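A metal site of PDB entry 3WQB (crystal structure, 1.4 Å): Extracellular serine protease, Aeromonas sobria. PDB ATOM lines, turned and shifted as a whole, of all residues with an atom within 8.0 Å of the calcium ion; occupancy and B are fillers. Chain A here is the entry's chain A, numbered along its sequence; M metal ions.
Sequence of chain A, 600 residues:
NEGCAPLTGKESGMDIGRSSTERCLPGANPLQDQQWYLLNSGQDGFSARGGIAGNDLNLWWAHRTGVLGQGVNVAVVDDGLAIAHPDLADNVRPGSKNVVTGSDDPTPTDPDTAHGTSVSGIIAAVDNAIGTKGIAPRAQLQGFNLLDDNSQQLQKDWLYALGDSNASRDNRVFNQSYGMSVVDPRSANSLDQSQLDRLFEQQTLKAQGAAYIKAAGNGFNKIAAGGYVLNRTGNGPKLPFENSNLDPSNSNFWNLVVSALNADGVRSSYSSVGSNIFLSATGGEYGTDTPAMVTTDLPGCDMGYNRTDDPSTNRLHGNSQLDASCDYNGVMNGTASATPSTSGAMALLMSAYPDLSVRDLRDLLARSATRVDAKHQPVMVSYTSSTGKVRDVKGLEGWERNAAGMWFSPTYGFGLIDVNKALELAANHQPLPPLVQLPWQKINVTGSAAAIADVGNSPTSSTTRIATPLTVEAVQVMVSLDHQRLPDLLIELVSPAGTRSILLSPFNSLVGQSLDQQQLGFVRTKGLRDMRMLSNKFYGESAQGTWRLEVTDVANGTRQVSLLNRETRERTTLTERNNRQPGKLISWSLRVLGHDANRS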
ATOM      1  N   ALA A  28      -3.632  -9.791   1.366  1.00  0.00           N
ATOM      2  CA  ALA A  28      -4.492  -9.463   2.498  1.00  0.00           C
ATOM      3  C   ALA A  28      -5.277 -10.672   2.969  1.00  0.00           C
ATOM      4  O   ALA A  28      -6.324 -10.539   3.592  1.00  0.00           O
ATOM      5  CB  ALA A  28      -5.447  -8.321   2.120  1.00  0.00           C
ATOM      6  N   ASN A  29      -4.779 -11.867   2.670  1.00  0.00           N
ATOM      7  CA  ASN A  29      -5.396 -13.094   3.170  1.00  0.00           C
ATOM      8  C   ASN A  29      -5.036 -13.255   4.641  1.00  0.00           C
ATOM      9  O   ASN A  29      -3.862 -13.335   4.982  1.00  0.00           O
ATOM     10  CB  ASN A  29      -4.903 -14.299   2.364  1.00  0.00           C
ATOM     11  CG  ASN A  29      -5.099 -14.106   0.877  1.00  0.00           C
ATOM     12  OD1 ASN A  29      -6.163 -14.402   0.339  1.00  0.00           O
ATOM     13  ND2 ASN A  29      -4.061 -13.596   0.193  1.00  0.00           N
ATOM     14  N   PRO A  30      -6.050 -13.271   5.526  1.00  0.00           N
ATOM     15  CA  PRO A  30      -5.741 -13.212   6.955  1.00  0.00           C
ATOM     16  C   PRO A  30      -4.882 -14.350   7.505  1.00  0.00           C
ATOM     17  O   PRO A  30      -4.211 -14.169   8.515  1.00  0.00           O
ATOM     18  CB  PRO A  30      -7.127 -13.188   7.615  1.00  0.00           C
ATOM     19  CG  PRO A  30      -8.012 -12.574   6.577  1.00  0.00           C
ATOM     20  CD  PRO A  30      -7.496 -13.150   5.282  1.00  0.00           C
ATOM     21  N   LEU A  31      -4.869 -15.506   6.837  1.00  0.00           N
ATOM     22  CA  LEU A  31      -4.111 -16.645   7.350  1.00  0.00           C
ATOM     23  C   LEU A  31      -2.753 -16.831   6.672  1.00  0.00           C
ATOM     24  O   LEU A  31      -2.011 -17.763   7.021  1.00  0.00           O
ATOM     25  CB  LEU A  31      -4.925 -17.940   7.241  1.00  0.00           C
ATOM     26  CG  LEU A  31      -6.308 -17.954   7.885  1.00  0.00           C
ATOM     27  CD1 LEU A  31      -6.974 -19.279   7.563  1.00  0.00           C
ATOM     28  CD2 LEU A  31      -6.225 -17.733   9.388  1.00  0.00           C
ATOM     29  N   GLN A  32      -2.398 -15.970   5.716  1.00  0.00           N
ATOM     30  CA  GLN A  32      -1.191 -16.231   4.935  1.00  0.00           C
ATOM     31  C   GLN A  32       0.101 -16.184   5.736  1.00  0.00           C
ATOM     32  O   GLN A  32       1.068 -16.857   5.396  1.00  0.00           O
ATOM     33  CB  GLN A  32      -1.110 -15.333   3.692  1.00  0.00           C
ATOM     34  CG  GLN A  32      -0.797 -13.861   3.929  1.00  0.00           C
ATOM     35  CD  GLN A  32      -0.770 -13.107   2.635  1.00  0.00           C
ATOM     36  OE1 GLN A  32      -1.775 -13.022   1.926  1.00  0.00           O
ATOM     37  NE2 GLN A  32       0.395 -12.552   2.287  1.00  0.00           N
ATOM     38  N   GLN A  35       0.971 -19.625   6.854  1.00  0.00           N
ATOM     39  CA  GLN A  35       1.363 -20.580   5.808  1.00  0.00           C
ATOM     40  C   GLN A  35       2.893 -20.549   5.705  1.00  0.00           C
ATOM     41  O   GLN A  35       3.461 -19.864   4.858  1.00  0.00           O
ATOM     42  CB  GLN A  35       0.721 -20.217   4.470  1.00  0.00           C
ATOM     43  CG  GLN A  35      -0.805 -20.293   4.466  1.00  0.00           C
ATOM     44  CD  GLN A  35      -1.377 -19.779   3.157  1.00  0.00           C
ATOM     45  OE1 GLN A  35      -1.869 -18.658   3.083  1.00  0.00           O
ATOM     46  NE2 GLN A  35      -1.291 -20.596   2.112  1.00  0.00           N
ATOM     47  N   HIS A  85     -16.331 -23.594  -2.394  1.00  0.00           N
ATOM     48  CA  HIS A  85     -15.575 -22.967  -1.313  1.00  0.00           C
ATOM     49  C   HIS A  85     -15.295 -21.514  -1.660  1.00  0.00           C
ATOM     50  O   HIS A  85     -14.861 -21.222  -2.778  1.00  0.00           O
ATOM     51  CB  HIS A  85     -14.240 -23.683  -1.110  1.00  0.00           C
ATOM     52  CG  HIS A  85     -13.577 -23.362   0.189  1.00  0.00           C
ATOM     53  ND1 HIS A  85     -13.012 -22.130   0.458  1.00  0.00           N
ATOM     54  CD2 HIS A  85     -13.433 -24.089   1.310  1.00  0.00           C
ATOM     55  CE1 HIS A  85     -12.527 -22.128   1.678  1.00  0.00           C
ATOM     56  NE2 HIS A  85     -12.761 -23.305   2.219  1.00  0.00           N
ATOM     57  N   PRO A  86     -15.526 -20.593  -0.711  1.00  0.00           N
ATOM     58  CA  PRO A  86     -15.355 -19.166  -1.026  1.00  0.00           C
ATOM     59  C   PRO A  86     -13.922 -18.779  -1.393  1.00  0.00           C
ATOM     60  O   PRO A  86     -13.720 -17.778  -2.110  1.00  0.00           O
ATOM     61  CB  PRO A  86     -15.799 -18.447   0.260  1.00  0.00           C
ATOM     62  CG  PRO A  86     -15.775 -19.481   1.330  1.00  0.00           C
ATOM     63  CD  PRO A  86     -16.056 -20.797   0.647  1.00  0.00           C
ATOM     64  N   ASP A  87     -12.948 -19.586  -0.966  1.00  0.00           N
ATOM     65  CA  ASP A  87     -11.549 -19.294  -1.267  1.00  0.00           C
ATOM     66  C   ASP A  87     -11.004 -20.168  -2.395  1.00  0.00           C
ATOM     67  O   ASP A  87      -9.801 -20.176  -2.621  1.00  0.00           O
ATOM     68  CB  ASP A  87     -10.685 -19.383  -0.009  1.00  0.00           C
ATOM     69  CG  ASP A  87      -9.613 -18.294   0.046  1.00  0.00           C
ATOM     70  OD1 ASP A  87      -9.740 -17.276  -0.683  1.00  0.00           O
ATOM     71  OD2 ASP A  87      -8.649 -18.433   0.827  1.00  0.00           O
ATOM     72  N   LEU A  88     -11.891 -20.891  -3.086  1.00  0.00           N
ATOM     73  CA  LEU A  88     -11.514 -21.694  -4.265  1.00  0.00           C
ATOM     74  C   LEU A  88     -12.320 -21.399  -5.525  1.00  0.00           C
ATOM     75  O   LEU A  88     -11.805 -21.516  -6.629  1.00  0.00           O
ATOM     76  CB  LEU A  88     -11.593 -23.193  -3.972  1.00  0.00           C
ATOM     77  CG  LEU A  88     -10.669 -23.727  -2.876  1.00  0.00           C
ATOM     78  CD1 LEU A  88     -11.026 -25.160  -2.519  1.00  0.00           C
ATOM     79  CD2 LEU A  88      -9.199 -23.632  -3.293  1.00  0.00           C
ATOM     80  N   ALA A 124      -3.867 -23.260  -5.054  1.00  0.00           N
ATOM     81  CA  ALA A 124      -4.545 -22.157  -5.705  1.00  0.00           C
ATOM     82  C   ALA A 124      -5.667 -21.502  -4.885  1.00  0.00           C
ATOM     83  O   ALA A 124      -6.638 -21.010  -5.454  1.00  0.00           O
ATOM     84  CB  ALA A 124      -5.069 -22.606  -7.071  1.00  0.00           C
ATOM     85  N   ALA A 125      -5.525 -21.449  -3.561  1.00  0.00           N
ATOM     86  CA  ALA A 125      -6.457 -20.626  -2.782  1.00  0.00           C
ATOM     87  C   ALA A 125      -6.411 -19.204  -3.341  1.00  0.00           C
ATOM     88  O   ALA A 125      -5.346 -18.672  -3.670  1.00  0.00           O
ATOM     89  CB  ALA A 125      -6.126 -20.667  -1.300  1.00  0.00           C
ATOM     90  N   VAL A 126      -7.589 -18.597  -3.441  1.00  0.00           N
ATOM     91  CA  VAL A 126      -7.725 -17.296  -4.084  1.00  0.00           C
ATOM     92  C   VAL A 126      -7.018 -16.192  -3.290  1.00  0.00           C
ATOM     93  O   VAL A 126      -7.043 -16.185  -2.055  1.00  0.00           O
ATOM     94  CB  VAL A 126      -9.223 -16.963  -4.319  1.00  0.00           C
ATOM     95  CG1 VAL A 126      -9.427 -15.587  -4.930  1.00  0.00           C
ATOM     96  CG2 VAL A 126      -9.832 -18.028  -5.201  1.00  0.00           C
ATOM     97  N   ASP A 127      -6.353 -15.290  -4.010  1.00  0.00           N
ATOM     98  CA  ASP A 127      -5.723 -14.134  -3.400  1.00  0.00           C
ATOM     99  C   ASP A 127      -6.767 -13.029  -3.219  1.00  0.00           C
ATOM    100  O   ASP A 127      -7.148 -12.357  -4.178  1.00  0.00           O
ATOM    101  CB  ASP A 127      -4.575 -13.653  -4.281  1.00  0.00           C
ATOM    102  CG  ASP A 127      -3.715 -12.602  -3.613  1.00  0.00           C
ATOM    103  OD1 ASP A 127      -3.758 -12.490  -2.363  1.00  0.00           O
ATOM    104  OD2 ASP A 127      -2.976 -11.908  -4.332  1.00  0.00           O
ATOM    105  N   ASN A 128      -7.230 -12.872  -1.986  1.00  0.00           N
ATOM    106  CA  ASN A 128      -8.328 -11.955  -1.687  1.00  0.00           C
ATOM    107  C   ASN A 128      -8.205 -11.506  -0.229  1.00  0.00           C
ATOM    108  O   ASN A 128      -7.088 -11.360   0.282  1.00  0.00           O
ATOM    109  CB  ASN A 128      -9.675 -12.612  -2.008  1.00  0.00           C
ATOM    110  CG  ASN A 128      -9.826 -13.972  -1.339  1.00  0.00           C
ATOM    111  OD1 ASN A 128      -9.101 -14.292  -0.403  1.00  0.00           O
ATOM    112  ND2 ASN A 128     -10.779 -14.775  -1.822  1.00  0.00           N
ATOM    113  N   ALA A 129      -9.335 -11.269   0.441  1.00  0.00           N
ATOM    114  CA  ALA A 129      -9.295 -10.803   1.834  1.00  0.00           C
ATOM    115  C   ALA A 129      -9.771 -11.854   2.831  1.00  0.00           C
ATOM    116  O   ALA A 129     -10.037 -11.548   4.014  1.00  0.00           O
ATOM    117  CB  ALA A 129     -10.094  -9.510   1.984  1.00  0.00           C
ATOM    118  N   ILE A 130      -9.884 -13.103   2.377  1.00  0.00           N
ATOM    119  CA  ILE A 130     -10.291 -14.212   3.239  1.00  0.00           C
ATOM    120  C   ILE A 130      -9.284 -15.361   3.189  1.00  0.00           C
ATOM    121  O   ILE A 130      -8.535 -15.499   2.232  1.00  0.00           O
ATOM    122  CB  ILE A 130     -11.713 -14.740   2.898  1.00  0.00           C
ATOM    123  CG1 ILE A 130     -11.785 -15.275   1.471  1.00  0.00           C
ATOM    124  CG2 ILE A 130     -12.767 -13.643   3.132  1.00  0.00           C
ATOM    125  CD1 ILE A 130     -13.041 -16.095   1.166  1.00  0.00           C
ATOM    126  N   GLY A 131      -9.261 -16.153   4.249  1.00  0.00           N
ATOM    127  CA  GLY A 131      -8.534 -17.419   4.233  1.00  0.00           C
ATOM    128  C   GLY A 131      -7.058 -17.321   3.948  1.00  0.00           C
ATOM    129  O   GLY A 131      -6.352 -16.472   4.504  1.00  0.00           O
ATOM    130  N   THR A 132      -6.607 -18.190   3.047  1.00  0.00           N
ATOM    131  CA  THR A 132      -5.200 -18.376   2.744  1.00  0.00           C
ATOM    132  C   THR A 132      -4.861 -17.824   1.356  1.00  0.00           C
ATOM    133  O   THR A 132      -5.746 -17.345   0.614  1.00  0.00           O
ATOM    134  CB  THR A 132      -4.845 -19.862   2.757  1.00  0.00           C
ATOM    135  OG1 THR A 132      -5.746 -20.572   1.897  1.00  0.00           O
ATOM    136  CG2 THR A 132      -4.911 -20.444   4.183  1.00  0.00           C
ATOM    137  N   LYS A 133      -3.584 -17.875   1.012  1.00  0.00           N
ATOM    138  CA  LYS A 133      -3.117 -17.519  -0.316  1.00  0.00           C
ATOM    139  C   LYS A 133      -2.500 -18.754  -0.959  1.00  0.00           C
ATOM    140  O   LYS A 133      -1.600 -19.366  -0.384  1.00  0.00           O
ATOM    141  CB  LYS A 133      -2.077 -16.394  -0.230  1.00  0.00           C
ATOM    142  CG  LYS A 133      -1.714 -15.759  -1.588  1.00  0.00           C
ATOM    143  CD  LYS A 133      -0.559 -14.766  -1.435  1.00  0.00           C
ATOM    144  CE  LYS A 133      -0.340 -13.975  -2.714  1.00  0.00           C
ATOM    145  NZ  LYS A 133       0.904 -13.133  -2.660  1.00  0.00           N
ATOM    146  N   GLY A 134      -2.967 -19.122  -2.137  1.00  0.00           N
ATOM    147  CA  GLY A 134      -2.345 -20.242  -2.853  1.00  0.00           C
ATOM    148  C   GLY A 134      -0.903 -19.961  -3.232  1.00  0.00           C
ATOM    149  O   GLY A 134      -0.474 -18.802  -3.332  1.00  0.00           O
ATOM    150  N   PRO A 137      -1.896 -18.562  -6.940  1.00  0.00           N
ATOM    151  CA  PRO A 137      -3.288 -18.170  -6.698  1.00  0.00           C
ATOM    152  C   PRO A 137      -4.053 -17.708  -7.929  1.00  0.00           C
ATOM    153  O   PRO A 137      -5.236 -17.367  -7.842  1.00  0.00           O
ATOM    154  CB  PRO A 137      -3.165 -17.049  -5.662  1.00  0.00           C
ATOM    155  CG  PRO A 137      -1.846 -16.439  -5.938  1.00  0.00           C
ATOM    156  CD  PRO A 137      -0.953 -17.567  -6.387  1.00  0.00           C
ATOM    157  N   THR A 296      -7.343 -24.594   2.705  1.00  0.00           N
ATOM    158  CA  THR A 296      -8.786 -24.645   2.598  1.00  0.00           C
ATOM    159  C   THR A 296      -9.334 -26.002   3.042  1.00  0.00           C
ATOM    160  O   THR A 296      -8.876 -27.056   2.590  1.00  0.00           O
ATOM    161  CB  THR A 296      -9.221 -24.364   1.157  1.00  0.00           C
ATOM    162  OG1 THR A 296      -8.479 -25.198   0.263  1.00  0.00           O
ATOM    163  CG2 THR A 296      -8.969 -22.916   0.780  1.00  0.00           C
ATOM    164  N   TYR A 328     -11.203 -23.387   6.933  1.00  0.00           N
ATOM    165  CA  TYR A 328      -9.754 -23.624   6.799  1.00  0.00           C
ATOM    166  C   TYR A 328      -9.315 -24.640   7.837  1.00  0.00           C
ATOM    167  O   TYR A 328      -9.980 -24.840   8.847  1.00  0.00           O
ATOM    168  CB  TYR A 328      -8.974 -22.284   6.921  1.00  0.00           C
ATOM    169  CG  TYR A 328      -9.586 -21.313   5.962  1.00  0.00           C
ATOM    170  CD1 TYR A 328      -9.260 -21.359   4.614  1.00  0.00           C
ATOM    171  CD2 TYR A 328     -10.591 -20.446   6.378  1.00  0.00           C
ATOM    172  CE1 TYR A 328      -9.887 -20.540   3.692  1.00  0.00           C
ATOM    173  CE2 TYR A 328     -11.234 -19.607   5.468  1.00  0.00           C
ATOM    174  CZ  TYR A 328     -10.878 -19.672   4.128  1.00  0.00           C
ATOM    175  OH  TYR A 328     -11.495 -18.868   3.210  1.00  0.00           O
HETATM  176 CA    CA M   1      -7.738 -16.195   0.136  1.00  0.00          CA
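The side-chain carboxylate (OD1) of Asp 127 is in hydrogen-bond range of the side-chain amide nitrogen (ND2) of Asn 29 (2.8 Å). ND2 of Asn 29 lies within hydrogen-bond range of OE1 of Gln 32 (2.9 Å). N of Asp 87 sits at hydrogen-bond distance from ND1 of His 85.
The calcium ion is bound by the backbone carbonyl oxygen (O) of Val 126 (2.3 Å), the backbone carbonyl oxygen (O) of Ile 130 (2.3 Å), the backbone carbonyl oxygen (O) of Thr 132 (2.3 Å), the side-chain amide oxygen (OD1) of Asn 29 (2.4 Å), the side-chain amide oxygen (OD1) of Asn 128 (2.4 Å), the side-chain carboxylate (OD1) of Asp 87 (2.4 Å) and the side-chain carboxylate (OD2) of Asp 87 (2.5 Å).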
